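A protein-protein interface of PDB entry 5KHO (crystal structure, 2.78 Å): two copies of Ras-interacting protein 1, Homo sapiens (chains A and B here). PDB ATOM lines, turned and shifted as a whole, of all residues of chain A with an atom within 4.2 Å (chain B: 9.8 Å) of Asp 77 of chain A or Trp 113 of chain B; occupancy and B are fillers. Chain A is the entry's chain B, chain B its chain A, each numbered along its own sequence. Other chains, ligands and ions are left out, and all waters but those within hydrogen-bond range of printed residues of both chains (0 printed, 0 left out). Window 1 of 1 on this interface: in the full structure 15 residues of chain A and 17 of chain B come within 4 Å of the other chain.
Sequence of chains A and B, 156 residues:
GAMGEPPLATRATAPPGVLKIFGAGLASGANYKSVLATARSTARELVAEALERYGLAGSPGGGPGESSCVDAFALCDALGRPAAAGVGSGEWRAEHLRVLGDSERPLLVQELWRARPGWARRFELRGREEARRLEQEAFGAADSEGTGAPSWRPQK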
ATOM      1  N   CYS A  76       9.464 -11.421 -21.699  1.00  0.00           N
ATOM      2  CA  CYS A  76      10.135 -12.702 -21.805  1.00  0.00           C
ATOM      3  C   CYS A  76      10.141 -13.495 -20.508  1.00  0.00           C
ATOM      4  O   CYS A  76      10.469 -12.957 -19.450  1.00  0.00           O
ATOM      5  CB  CYS A  76      11.562 -12.505 -22.310  1.00  0.00           C
ATOM      6  SG  CYS A  76      11.632 -11.632 -23.889  1.00  0.00           S
ATOM      7  N   ASP A  77       9.764 -14.773 -20.618  1.00  0.00           N
ATOM      8  CA  ASP A  77       9.903 -15.753 -19.551  1.00  0.00           C
ATOM      9  C   ASP A  77      11.299 -16.348 -19.681  1.00  0.00           C
ATOM     10  O   ASP A  77      11.538 -17.224 -20.516  1.00  0.00           O
ATOM     11  CB  ASP A  77       8.805 -16.824 -19.670  1.00  0.00           C
ATOM     12  CG  ASP A  77       8.630 -17.669 -18.391  1.00  0.00           C
ATOM     13  OD1 ASP A  77       9.436 -17.587 -17.425  1.00  0.00           O
ATOM     14  OD2 ASP A  77       7.657 -18.444 -18.361  1.00  0.00           O
ATOM     15  N   ALA A  78      12.224 -15.844 -18.873  1.00  0.00           N
ATOM     16  CA  ALA A  78      13.638 -16.252 -18.934  1.00  0.00           C
ATOM     17  C   ALA A  78      14.004 -17.312 -17.894  1.00  0.00           C
ATOM     18  O   ALA A  78      13.359 -17.410 -16.840  1.00  0.00           O
ATOM     19  CB  ALA A  78      14.540 -15.038 -18.787  1.00  0.00           C
ATOM     20  N   LEU A  79      15.041 -18.094 -18.202  1.00  0.00           N
ATOM     21  CA  LEU A  79      15.515 -19.194 -17.351  1.00  0.00           C
ATOM     22  C   LEU A  79      17.036 -19.353 -17.418  1.00  0.00           C
ATOM     23  O   LEU A  79      17.663 -19.017 -18.428  1.00  0.00           O
ATOM     24  CB  LEU A  79      14.892 -20.524 -17.792  1.00  0.00           C
ATOM     25  CG  LEU A  79      13.404 -20.731 -18.040  1.00  0.00           C
ATOM     26  CD1 LEU A  79      13.251 -21.925 -18.954  1.00  0.00           C
ATOM     27  CD2 LEU A  79      12.652 -20.956 -16.742  1.00  0.00           C
ATOM     28  N   HIS A  96      18.007 -19.735 -21.538  1.00  0.00           N
ATOM     29  CA  HIS A  96      16.935 -19.854 -22.527  1.00  0.00           C
ATOM     30  C   HIS A  96      15.855 -18.859 -22.155  1.00  0.00           C
ATOM     31  O   HIS A  96      15.699 -18.525 -20.986  1.00  0.00           O
ATOM     32  CB  HIS A  96      16.363 -21.284 -22.566  1.00  0.00           C
ATOM     33  CG  HIS A  96      15.224 -21.464 -23.528  1.00  0.00           C
ATOM     34  ND1 HIS A  96      15.388 -21.422 -24.898  1.00  0.00           N
ATOM     35  CD2 HIS A  96      13.903 -21.678 -23.316  1.00  0.00           C
ATOM     36  CE1 HIS A  96      14.216 -21.594 -25.487  1.00  0.00           C
ATOM     37  NE2 HIS A  96      13.299 -21.755 -24.550  1.00  0.00           N
ATOM     38  N   LEU A  97      15.124 -18.369 -23.150  1.00  0.00           N
ATOM     39  CA  LEU A  97      13.955 -17.528 -22.894  1.00  0.00           C
ATOM     40  C   LEU A  97      12.792 -17.838 -23.830  1.00  0.00           C
ATOM     41  O   LEU A  97      12.953 -18.543 -24.822  1.00  0.00           O
ATOM     42  CB  LEU A  97      14.324 -16.033 -22.933  1.00  0.00           C
ATOM     43  CG  LEU A  97      14.817 -15.343 -24.209  1.00  0.00           C
ATOM     44  CD1 LEU A  97      13.685 -15.055 -25.191  1.00  0.00           C
ATOM     45  CD2 LEU A  97      15.494 -14.046 -23.815  1.00  0.00           C
ATOM     46  N   ARG A  98      11.628 -17.285 -23.508  1.00  0.00           N
ATOM     47  CA  ARG A  98      10.441 -17.432 -24.328  1.00  0.00           C
ATOM     48  C   ARG A  98       9.719 -16.103 -24.394  1.00  0.00           C
ATOM     49  O   ARG A  98       9.487 -15.477 -23.362  1.00  0.00           O
ATOM     50  CB  ARG A  98       9.534 -18.488 -23.722  1.00  0.00           C
ATOM     51  CG  ARG A  98       8.327 -18.824 -24.553  1.00  0.00           C
ATOM     52  CD  ARG A  98       7.426 -19.775 -23.791  1.00  0.00           C
ATOM     53  NE  ARG A  98       6.039 -19.372 -23.977  1.00  0.00           N
ATOM     54  CZ  ARG A  98       5.308 -18.750 -23.066  1.00  0.00           C
ATOM     55  NH1 ARG A  98       5.802 -18.482 -21.872  1.00  0.00           N
ATOM     56  NH2 ARG A  98       4.069 -18.408 -23.348  1.00  0.00           N
ATOM     57  N   LEU A 100       6.527 -14.182 -24.609  1.00  0.00           N
ATOM     58  CA  LEU A 100       5.080 -14.249 -24.447  1.00  0.00           C
ATOM     59  C   LEU A 100       4.383 -13.598 -25.634  1.00  0.00           C
ATOM     60  O   LEU A 100       4.836 -12.559 -26.126  1.00  0.00           O
ATOM     61  CB  LEU A 100       4.653 -13.548 -23.150  1.00  0.00           C
ATOM     62  CG  LEU A 100       4.670 -14.323 -21.817  1.00  0.00           C
ATOM     63  CD1 LEU A 100       6.053 -14.833 -21.429  1.00  0.00           C
ATOM     64  CD2 LEU A 100       4.082 -13.474 -20.692  1.00  0.00           C
ATOM     65  N   VAL A 109       1.195 -17.237 -16.236  1.00  0.00           N
ATOM     66  CA  VAL A 109       2.445 -17.838 -16.726  1.00  0.00           C
ATOM     67  C   VAL A 109       3.434 -18.089 -15.578  1.00  0.00           C
ATOM     68  O   VAL A 109       4.009 -19.181 -15.493  1.00  0.00           O
ATOM     69  CB  VAL A 109       3.087 -17.007 -17.886  1.00  0.00           C
ATOM     70  CG1 VAL A 109       4.538 -17.414 -18.175  1.00  0.00           C
ATOM     71  CG2 VAL A 109       2.243 -17.104 -19.155  1.00  0.00           C
ATOM     72  N   ARG A 114       6.859 -23.483 -13.504  1.00  0.00           N
ATOM     73  CA  ARG A 114       8.062 -23.297 -12.707  1.00  0.00           C
ATOM     74  C   ARG A 114       9.231 -23.761 -13.518  1.00  0.00           C
ATOM     75  O   ARG A 114       9.070 -24.593 -14.397  1.00  0.00           O
ATOM     76  CB  ARG A 114       7.986 -24.117 -11.419  1.00  0.00           C
ATOM     77  CG  ARG A 114       7.685 -23.267 -10.207  1.00  0.00           C
ATOM     78  CD  ARG A 114       6.614 -23.912  -9.358  1.00  0.00           C
ATOM     79  NE  ARG A 114       6.203 -23.043  -8.254  1.00  0.00           N
ATOM     80  CZ  ARG A 114       5.318 -22.051  -8.344  1.00  0.00           C
ATOM     81  NH1 ARG A 114       4.721 -21.751  -9.498  1.00  0.00           N
ATOM     82  NH2 ARG A 114       5.033 -21.349  -7.259  1.00  0.00           N
ATOM     83  N   ARG A 121      14.358 -18.207 -12.476  1.00  0.00           N
ATOM     84  CA  ARG A 121      13.391 -17.757 -13.459  1.00  0.00           C
ATOM     85  C   ARG A 121      12.909 -16.343 -13.141  1.00  0.00           C
ATOM     86  O   ARG A 121      12.453 -16.074 -12.021  1.00  0.00           O
ATOM     87  CB  ARG A 121      12.226 -18.725 -13.489  1.00  0.00           C
ATOM     88  CG  ARG A 121      11.115 -18.369 -14.440  1.00  0.00           C
ATOM     89  CD  ARG A 121       9.845 -19.074 -14.030  1.00  0.00           C
ATOM     90  NE  ARG A 121       8.814 -18.976 -15.056  1.00  0.00           N
ATOM     91  CZ  ARG A 121       7.524 -19.235 -14.850  1.00  0.00           C
ATOM     92  NH1 ARG A 121       7.093 -19.604 -13.644  1.00  0.00           N
ATOM     93  NH2 ARG A 121       6.658 -19.120 -15.850  1.00  0.00           N
ATOM     94  N   ARG A 122      13.017 -15.457 -14.132  1.00  0.00           N
ATOM     95  CA  ARG A 122      12.573 -14.073 -14.016  1.00  0.00           C
ATOM     96  C   ARG A 122      11.939 -13.584 -15.318  1.00  0.00           C
ATOM     97  O   ARG A 122      12.235 -14.124 -16.387  1.00  0.00           O
ATOM     98  CB  ARG A 122      13.735 -13.158 -13.600  1.00  0.00           C
ATOM     99  CG  ARG A 122      14.765 -12.872 -14.685  1.00  0.00           C
ATOM    100  CD  ARG A 122      16.007 -12.219 -14.118  1.00  0.00           C
ATOM    101  NE  ARG A 122      16.895 -11.753 -15.184  1.00  0.00           N
ATOM    102  CZ  ARG A 122      18.046 -11.107 -14.996  1.00  0.00           C
ATOM    103  NH1 ARG A 122      18.756 -10.721 -16.045  1.00  0.00           N
ATOM    104  NH2 ARG A 122      18.498 -10.841 -13.773  1.00  0.00           N
ATOM    105  N   ASP B  77       0.104 -27.095 -24.212  1.00  0.00           N
ATOM    106  CA  ASP B  77       0.689 -27.407 -22.910  1.00  0.00           C
ATOM    107  C   ASP B  77      -0.390 -27.363 -21.815  1.00  0.00           C
ATOM    108  O   ASP B  77      -0.704 -26.295 -21.282  1.00  0.00           O
ATOM    109  CB  ASP B  77       1.874 -26.464 -22.611  1.00  0.00           C
ATOM    110  CG  ASP B  77       2.711 -26.908 -21.414  1.00  0.00           C
ATOM    111  OD1 ASP B  77       2.500 -28.012 -20.867  1.00  0.00           O
ATOM    112  OD2 ASP B  77       3.597 -26.135 -21.011  1.00  0.00           O
ATOM    113  N   LEU B  79      -2.350 -28.274 -18.164  1.00  0.00           N
ATOM    114  CA  LEU B  79      -2.134 -28.434 -16.718  1.00  0.00           C
ATOM    115  C   LEU B  79      -3.446 -28.737 -15.986  1.00  0.00           C
ATOM    116  O   LEU B  79      -4.487 -28.130 -16.270  1.00  0.00           O
ATOM    117  CB  LEU B  79      -1.529 -27.165 -16.109  1.00  0.00           C
ATOM    118  CG  LEU B  79      -0.313 -26.448 -16.696  1.00  0.00           C
ATOM    119  CD1 LEU B  79      -0.372 -24.984 -16.312  1.00  0.00           C
ATOM    120  CD2 LEU B  79       0.982 -27.059 -16.202  1.00  0.00           C
ATOM    121  N   ARG B  98      -2.039 -23.749 -22.456  1.00  0.00           N
ATOM    122  CA  ARG B  98      -1.439 -22.793 -23.361  1.00  0.00           C
ATOM    123  C   ARG B  98      -1.196 -23.429 -24.730  1.00  0.00           C
ATOM    124  O   ARG B  98      -0.567 -24.486 -24.830  1.00  0.00           O
ATOM    125  CB  ARG B  98      -0.145 -22.271 -22.769  1.00  0.00           C
ATOM    126  CG  ARG B  98       0.689 -21.501 -23.755  1.00  0.00           C
ATOM    127  CD  ARG B  98       1.914 -20.966 -23.077  1.00  0.00           C
ATOM    128  NE  ARG B  98       3.104 -21.811 -23.202  1.00  0.00           N
ATOM    129  CZ  ARG B  98       3.915 -21.842 -24.259  1.00  0.00           C
ATOM    130  NH1 ARG B  98       3.644 -21.138 -25.355  1.00  0.00           N
ATOM    131  NH2 ARG B  98       4.995 -22.604 -24.228  1.00  0.00           N
ATOM    132  N   LEU B 100       0.746 -23.685 -28.002  1.00  0.00           N
ATOM    133  CA  LEU B 100       2.113 -23.401 -28.428  1.00  0.00           C
ATOM    134  C   LEU B 100       2.163 -22.711 -29.776  1.00  0.00           C
ATOM    135  O   LEU B 100       1.432 -23.074 -30.699  1.00  0.00           O
ATOM    136  CB  LEU B 100       2.950 -24.676 -28.476  1.00  0.00           C
ATOM    137  CG  LEU B 100       3.847 -24.949 -27.278  1.00  0.00           C
ATOM    138  CD1 LEU B 100       3.063 -25.425 -26.066  1.00  0.00           C
ATOM    139  CD2 LEU B 100       4.902 -25.971 -27.683  1.00  0.00           C
ATOM    140  N   GLU B 104       7.803 -22.425 -31.722  1.00  0.00           N
ATOM    141  CA  GLU B 104       8.257 -22.950 -30.427  1.00  0.00           C
ATOM    142  C   GLU B 104       8.759 -24.385 -30.503  1.00  0.00           C
ATOM    143  O   GLU B 104       8.221 -25.209 -31.254  1.00  0.00           O
ATOM    144  CB  GLU B 104       7.154 -22.863 -29.371  1.00  0.00           C
ATOM    145  CG  GLU B 104       6.896 -21.471 -28.830  1.00  0.00           C
ATOM    146  CD  GLU B 104       5.985 -21.486 -27.618  1.00  0.00           C
ATOM    147  OE1 GLU B 104       6.471 -21.852 -26.522  1.00  0.00           O
ATOM    148  OE2 GLU B 104       4.793 -21.117 -27.759  1.00  0.00           O
ATOM    149  N   ARG B 105       9.787 -24.660 -29.703  1.00  0.00           N
ATOM    150  CA  ARG B 105      10.429 -25.963 -29.649  1.00  0.00           C
ATOM    151  C   ARG B 105       9.866 -26.675 -28.423  1.00  0.00           C
ATOM    152  O   ARG B 105      10.185 -26.288 -27.294  1.00  0.00           O
ATOM    153  CB  ARG B 105      11.958 -25.807 -29.602  1.00  0.00           C
ATOM    154  CG  ARG B 105      12.506 -24.879 -30.687  1.00  0.00           C
ATOM    155  CD  ARG B 105      14.019 -24.775 -30.659  1.00  0.00           C
ATOM    156  NE  ARG B 105      14.516 -23.620 -29.914  1.00  0.00           N
ATOM    157  CZ  ARG B 105      15.690 -23.572 -29.279  1.00  0.00           C
ATOM    158  NH1 ARG B 105      16.505 -24.628 -29.267  1.00  0.00           N
ATOM    159  NH2 ARG B 105      16.051 -22.466 -28.637  1.00  0.00           N
ATOM    160  N   PRO B 106       8.990 -27.687 -28.634  1.00  0.00           N
ATOM    161  CA  PRO B 106       8.244 -28.282 -27.512  1.00  0.00           C
ATOM    162  C   PRO B 106       9.070 -29.147 -26.563  1.00  0.00           C
ATOM    163  O   PRO B 106       8.675 -29.310 -25.403  1.00  0.00           O
ATOM    164  CB  PRO B 106       7.172 -29.129 -28.199  1.00  0.00           C
ATOM    165  CG  PRO B 106       7.179 -28.710 -29.631  1.00  0.00           C
ATOM    166  CD  PRO B 106       8.569 -28.266 -29.921  1.00  0.00           C
ATOM    167  N   LEU B 107      10.192 -29.687 -27.049  1.00  0.00           N
ATOM    168  CA  LEU B 107      11.127 -30.458 -26.221  1.00  0.00           C
ATOM    169  C   LEU B 107      11.649 -29.593 -25.089  1.00  0.00           C
ATOM    170  O   LEU B 107      11.677 -30.034 -23.936  1.00  0.00           O
ATOM    171  CB  LEU B 107      12.302 -30.995 -27.052  1.00  0.00           C
ATOM    172  CG  LEU B 107      13.169 -32.202 -26.633  1.00  0.00           C
ATOM    173  CD1 LEU B 107      13.991 -31.974 -25.378  1.00  0.00           C
ATOM    174  CD2 LEU B 107      12.354 -33.483 -26.502  1.00  0.00           C
ATOM    175  N   LEU B 108      12.045 -28.363 -25.420  1.00  0.00           N
ATOM    176  CA  LEU B 108      12.483 -27.387 -24.418  1.00  0.00           C
ATOM    177  C   LEU B 108      11.363 -26.926 -23.483  1.00  0.00           C
ATOM    178  O   LEU B 108      11.603 -26.772 -22.289  1.00  0.00           O
ATOM    179  CB  LEU B 108      13.170 -26.181 -25.069  1.00  0.00           C
ATOM    180  CG  LEU B 108      14.383 -26.318 -26.009  1.00  0.00           C
ATOM    181  CD1 LEU B 108      15.134 -24.995 -25.967  1.00  0.00           C
ATOM    182  CD2 LEU B 108      15.339 -27.474 -25.706  1.00  0.00           C
ATOM    183  N   VAL B 109      10.154 -26.715 -24.023  1.00  0.00           N
ATOM    184  CA  VAL B 109       8.958 -26.387 -23.225  1.00  0.00           C
ATOM    185  C   VAL B 109       8.773 -27.471 -22.165  1.00  0.00           C
ATOM    186  O   VAL B 109       8.614 -27.156 -20.986  1.00  0.00           O
ATOM    187  CB  VAL B 109       7.680 -26.189 -24.115  1.00  0.00           C
ATOM    188  CG1 VAL B 109       6.377 -26.138 -23.308  1.00  0.00           C
ATOM    189  CG2 VAL B 109       7.802 -24.928 -24.972  1.00  0.00           C
ATOM    190  N   GLN B 110       8.844 -28.739 -22.584  1.00  0.00           N
ATOM    191  CA  GLN B 110       8.767 -29.875 -21.658  1.00  0.00           C
ATOM    192  C   GLN B 110       9.921 -29.909 -20.659  1.00  0.00           C
ATOM    193  O   GLN B 110       9.693 -29.943 -19.454  1.00  0.00           O
ATOM    194  CB  GLN B 110       8.673 -31.211 -22.410  1.00  0.00           C
ATOM    195  CG  GLN B 110       8.695 -32.441 -21.505  1.00  0.00           C
ATOM    196  CD  GLN B 110       7.771 -33.542 -21.978  1.00  0.00           C
ATOM    197  OE1 GLN B 110       8.223 -34.572 -22.481  1.00  0.00           O
ATOM    198  NE2 GLN B 110       6.463 -33.330 -21.825  1.00  0.00           N
ATOM    199  N   GLU B 111      11.150 -29.897 -21.161  1.00  0.00           N
ATOM    200  CA  GLU B 111      12.291 -30.193 -20.312  1.00  0.00           C
ATOM    201  C   GLU B 111      12.728 -29.017 -19.413  1.00  0.00           C
ATOM    202  O   GLU B 111      13.326 -29.243 -18.357  1.00  0.00           O
ATOM    203  CB  GLU B 111      13.452 -30.795 -21.132  1.00  0.00           C
ATOM    204  N   LEU B 112      12.407 -27.785 -19.807  1.00  0.00           N
ATOM    205  CA  LEU B 112      12.894 -26.587 -19.098  1.00  0.00           C
ATOM    206  C   LEU B 112      11.915 -25.960 -18.113  1.00  0.00           C
ATOM    207  O   LEU B 112      12.301 -25.119 -17.287  1.00  0.00           O
ATOM    208  CB  LEU B 112      13.384 -25.524 -20.081  1.00  0.00           C
ATOM    209  CG  LEU B 112      14.738 -25.798 -20.753  1.00  0.00           C
ATOM    210  CD1 LEU B 112      15.094 -24.685 -21.728  1.00  0.00           C
ATOM    211  CD2 LEU B 112      15.850 -25.996 -19.726  1.00  0.00           C
ATOM    212  N   TRP B 113      10.650 -26.353 -18.220  1.00  0.00           N
ATOM    213  CA  TRP B 113       9.626 -25.920 -17.294  1.00  0.00           C
ATOM    214  C   TRP B 113       8.960 -27.128 -16.676  1.00  0.00           C
ATOM    215  O   TRP B 113       8.999 -28.224 -17.235  1.00  0.00           O
ATOM    216  CB  TRP B 113       8.578 -25.068 -17.996  1.00  0.00           C
ATOM    217  CG  TRP B 113       9.010 -23.664 -18.301  1.00  0.00           C
ATOM    218  CD1 TRP B 113       9.030 -22.610 -17.442  1.00  0.00           C
ATOM    219  CD2 TRP B 113       9.456 -23.159 -19.564  1.00  0.00           C
ATOM    220  NE1 TRP B 113       9.464 -21.474 -18.088  1.00  0.00           N
ATOM    221  CE2 TRP B 113       9.742 -21.786 -19.388  1.00  0.00           C
ATOM    222  CE3 TRP B 113       9.659 -23.736 -20.824  1.00  0.00           C
ATOM    223  CZ2 TRP B 113      10.208 -20.976 -20.423  1.00  0.00           C
ATOM    224  CZ3 TRP B 113      10.117 -22.922 -21.863  1.00  0.00           C
ATOM    225  CH2 TRP B 113      10.387 -21.558 -21.650  1.00  0.00           C
ATOM    226  N   ARG B 114       8.368 -26.922 -15.505  1.00  0.00           N
ATOM    227  CA  ARG B 114       7.511 -27.911 -14.877  1.00  0.00           C
ATOM    228  C   ARG B 114       6.208 -27.251 -14.428  1.00  0.00           C
ATOM    229  O   ARG B 114       6.101 -26.017 -14.378  1.00  0.00           O
ATOM    230  CB  ARG B 114       8.238 -28.632 -13.732  1.00  0.00           C
ATOM    231  CG  ARG B 114       8.662 -27.772 -12.556  1.00  0.00           C
ATOM    232  CD  ARG B 114       8.991 -28.647 -11.352  1.00  0.00           C
ATOM    233  NE  ARG B 114       8.559 -28.033 -10.091  1.00  0.00           N
ATOM    234  CZ  ARG B 114       9.351 -27.367  -9.248  1.00  0.00           C
ATOM    235  NH1 ARG B 114       8.833 -26.848  -8.142  1.00  0.00           N
ATOM    236  NH2 ARG B 114      10.652 -27.217  -9.501  1.00  0.00           N
ATOM    237  N   ALA B 115       5.208 -28.077 -14.143  1.00  0.00           N
ATOM    238  CA  ALA B 115       3.970 -27.608 -13.544  1.00  0.00           C
ATOM    239  C   ALA B 115       4.210 -27.171 -12.095  1.00  0.00           C
ATOM    240  O   ALA B 115       5.264 -27.487 -11.508  1.00  0.00           O
ATOM    241  CB  ALA B 115       2.934 -28.714 -13.596  1.00  0.00           C
ATOM    242  N   ARG B 116       3.236 -26.436 -11.535  1.00  0.00           N
ATOM    243  CA  ARG B 116       3.096 -26.254 -10.081  1.00  0.00           C
ATOM    244  C   ARG B 116       3.253 -27.609  -9.387  1.00  0.00           C
ATOM    245  O   ARG B 116       2.774 -28.628  -9.915  1.00  0.00           O
ATOM    246  CB  ARG B 116       1.708 -25.733  -9.706  1.00  0.00           C
ATOM    247  CG  ARG B 116       1.248 -24.468 -10.385  1.00  0.00           C
ATOM    248  CD  ARG B 116      -0.127 -24.053  -9.889  1.00  0.00           C
ATOM    249  NE  ARG B 116      -0.072 -23.229  -8.676  1.00  0.00           N
ATOM    250  CZ  ARG B 116      -0.664 -23.511  -7.514  1.00  0.00           C
ATOM    251  NH1 ARG B 116      -1.387 -24.617  -7.345  1.00  0.00           N
ATOM    252  NH2 ARG B 116      -0.535 -22.663  -6.504  1.00  0.00           N
ATOM    253  N   TRP B 119       0.410 -30.278  -9.315  1.00  0.00           N
ATOM    254  CA  TRP B 119      -0.241 -30.266 -10.635  1.00  0.00           C
ATOM    255  C   TRP B 119       0.420 -31.197 -11.647  1.00  0.00           C
ATOM    256  O   TRP B 119       1.640 -31.360 -11.657  1.00  0.00           O
ATOM    257  CB  TRP B 119      -0.306 -28.839 -11.196  1.00  0.00           C
ATOM    258  CG  TRP B 119      -1.254 -27.921 -10.461  1.00  0.00           C
ATOM    259  CD1 TRP B 119      -1.395 -27.794  -9.101  1.00  0.00           C
ATOM    260  CD2 TRP B 119      -2.171 -26.984 -11.040  1.00  0.00           C
ATOM    261  NE1 TRP B 119      -2.352 -26.855  -8.802  1.00  0.00           N
ATOM    262  CE2 TRP B 119      -2.843 -26.337  -9.969  1.00  0.00           C
ATOM    263  CE3 TRP B 119      -2.493 -26.626 -12.353  1.00  0.00           C
ATOM    264  CZ2 TRP B 119      -3.815 -25.347 -10.175  1.00  0.00           C
ATOM    265  CZ3 TRP B 119      -3.470 -25.643 -12.557  1.00  0.00           C
ATOM    266  CH2 TRP B 119      -4.119 -25.017 -11.469  1.00  0.00           C
ATOM    267  N   ARG B 121       0.827 -32.385 -15.876  1.00  0.00           N
ATOM    268  CA  ARG B 121       1.112 -31.686 -17.135  1.00  0.00           C
ATOM    269  C   ARG B 121       1.192 -32.658 -18.307  1.00  0.00           C
ATOM    270  O   ARG B 121       1.770 -33.727 -18.178  1.00  0.00           O
ATOM    271  CB  ARG B 121       2.407 -30.886 -16.992  1.00  0.00           C
ATOM    272  CG  ARG B 121       2.758 -29.975 -18.145  1.00  0.00           C
ATOM    273  CD  ARG B 121       4.145 -29.389 -17.932  1.00  0.00           C
ATOM    274  NE  ARG B 121       4.487 -28.391 -18.940  1.00  0.00           N
ATOM    275  CZ  ARG B 121       5.723 -28.095 -19.338  1.00  0.00           C
ATOM    276  NH1 ARG B 121       5.902 -27.166 -20.265  1.00  0.00           N
ATOM    277  NH2 ARG B 121       6.782 -28.714 -18.825  1.00  0.00           N
ATOM    278  N   ARG B 122       0.603 -32.288 -19.438  1.00  0.00           N
ATOM    279  CA  ARG B 122       0.678 -33.096 -20.658  1.00  0.00           C
ATOM    280  C   ARG B 122       0.591 -32.232 -21.917  1.00  0.00           C
ATOM    281  O   ARG B 122       0.077 -31.118 -21.874  1.00  0.00           O
ATOM    282  CB  ARG B 122      -0.414 -34.180 -20.668  1.00  0.00           C
ATOM    283  CG  ARG B 122      -1.829 -33.634 -20.554  1.00  0.00           C
ATOM    284  CD  ARG B 122      -2.877 -34.558 -21.136  1.00  0.00           C
ATOM    285  NE  ARG B 122      -3.163 -35.700 -20.274  1.00  0.00           N
ATOM    286  CZ  ARG B 122      -4.340 -36.317 -20.197  1.00  0.00           C
ATOM    287  NH1 ARG B 122      -4.482 -37.352 -19.379  1.00  0.00           N
ATOM    288  NH2 ARG B 122      -5.376 -35.905 -20.924  1.00  0.00           N
ATOM    289  N   PHE B 123       1.110 -32.744 -23.031  1.00  0.00           N
ATOM    290  CA  PHE B 123       0.870 -32.135 -24.342  1.00  0.00           C
ATOM    291  C   PHE B 123      -0.424 -32.686 -24.925  1.00  0.00           C
ATOM    292  O   PHE B 123      -0.732 -33.870 -24.749  1.00  0.00           O
ATOM    293  CB  PHE B 123       2.036 -32.374 -25.302  1.00  0.00           C
ATOM    294  CG  PHE B 123       3.249 -31.540 -25.010  1.00  0.00           C
ATOM    295  CD1 PHE B 123       3.168 -30.143 -24.963  1.00  0.00           C
ATOM    296  CD2 PHE B 123       4.484 -32.145 -24.804  1.00  0.00           C
ATOM    297  CE1 PHE B 123       4.295 -29.372 -24.700  1.00  0.00           C
ATOM    298  CE2 PHE B 123       5.617 -31.382 -24.538  1.00  0.00           C
ATOM    299  CZ  PHE B 123       5.525 -29.994 -24.487  1.00  0.00           C
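The guanidinium group (NE) of Arg 98 of chain A lies within salt-bridge range of the side-chain carboxylate (OE1) of Glu 104 of chain B (3.6 Å). The guanidinium group of Arg 98 of chain A lies close to the guanidinium group of Arg 98 of chain B, 3.3 Å away. O of Arg 114 of chain A sits at hydrogen-bond distance from N of Arg 114 of chain B (2.7 Å).
OD2 of Asp 77 of chain A lies within salt-bridge range of NH1 of Arg 98 of chain A, at 3.97 Å. O of His 96 of chain A lies within hydrogen-bond range of N of Leu 79 of chain A, 2.9 Å away. The backbone carbonyl oxygen (O) of Trp 113 of chain B sits at hydrogen-bond distance from the guanidinium group (NH2) of Arg 121 of chain B (2.8 Å). O of Arg 98 of chain B is in hydrogen-bond range of N of Asp 77 of chain B (2.8 Å). NH2 of Arg 121 of chain A is in salt-bridge range of OD2 of Asp 77 of chain A, at 2.8 Å. O of Val 109 of chain A sits at hydrogen-bond distance from NH2 of Arg 121 of chain A (2.7 Å).
NE1 of Trp 113 of chain B touches OD2 of Asp 77 of chain A (3.5 Å). Leu 79 of chain A touches Leu 112 of chain B (CD1 to O, 3.7 Å). Leu 79 of chain A touches Trp 113 of chain B. His 96 of chain A touches Arg 105 of chain B (CE1 to NH2, 3.7 Å). CD1 of Leu 108 of chain B touches CE1 of His 96 of chain A (3.6 Å). CD1 of Leu 112 of chain B touches CD2 of His 96 of chain A, at 3.6 Å. Trp 113 of chain B touches His 96 of chain A (CH2 to CD2, 3.9 Å). CB of Arg 98 of chain A touches CH2 of Trp 113 of chain B, 3.8 Å away. CA of Trp 113 of chain B touches O of Arg 114 of chain A, at 3.2 Å. Arg 121 of chain A touches Trp 113 of chain B (NE to NE1, 3.98 Å).
Asp 77 of chain A touches just one residue of chain B: Trp 113. Printed residues of chain A within 4 Å of Trp 113 of chain B: Asp 77, Leu 79, His 96, Arg 98, Arg 114 and Arg 121. No residue of chain B comes within 4 Å of Cys 76 of chain A. No residue of chain B comes within 4 Å of Ala 78 of chain A. Printed residues of chain A within 4 Å of Leu 112 of chain B: Leu 79 and His 96. Of the printed residues of chain B, Arg 121 of chain A touches Trp 113 (3.98 Å). The nearest residue of chain B that does not touch Asp 77 of chain A is Arg 98 of chain B (7.4 Å). The nearest printed residue of chain A that does not touch Trp 113 of chain B is Leu 97 of chain A (4.9 Å). The nearest printed residue of chain B that does not touch His 96 of chain A is Val 109 of chain B (5.9 Å).
Printed residues of chain A that touch a printed residue of chain B: Asp 77, Leu 79, His 96, Arg 98, Arg 114 and Arg 121. Along chain A the printed residues that touch a printed residue of chain B span positions 77 to 121. Hydrophobic or aromatic side chains of chain B that line the printed part of chain A: Leu 108, Leu 112 and Trp 113. Along chain B the printed residues that touch a printed residue of chain A span positions 98 to 114. Among the printed residues, 13 pairs touch across the chains.
Arg 98 of chain B touches its own counterpart, Arg 98 of chain A. Arg 114 of chain A touches its own counterpart, Arg 114 of chain B. Positions printed for both chains: 77, 79, 98, 100, 109, 114, 121 and 122. Of the 13 pairs that touch across the chains among the printed residues, 2 have their exchanged pair printed and touching as well.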
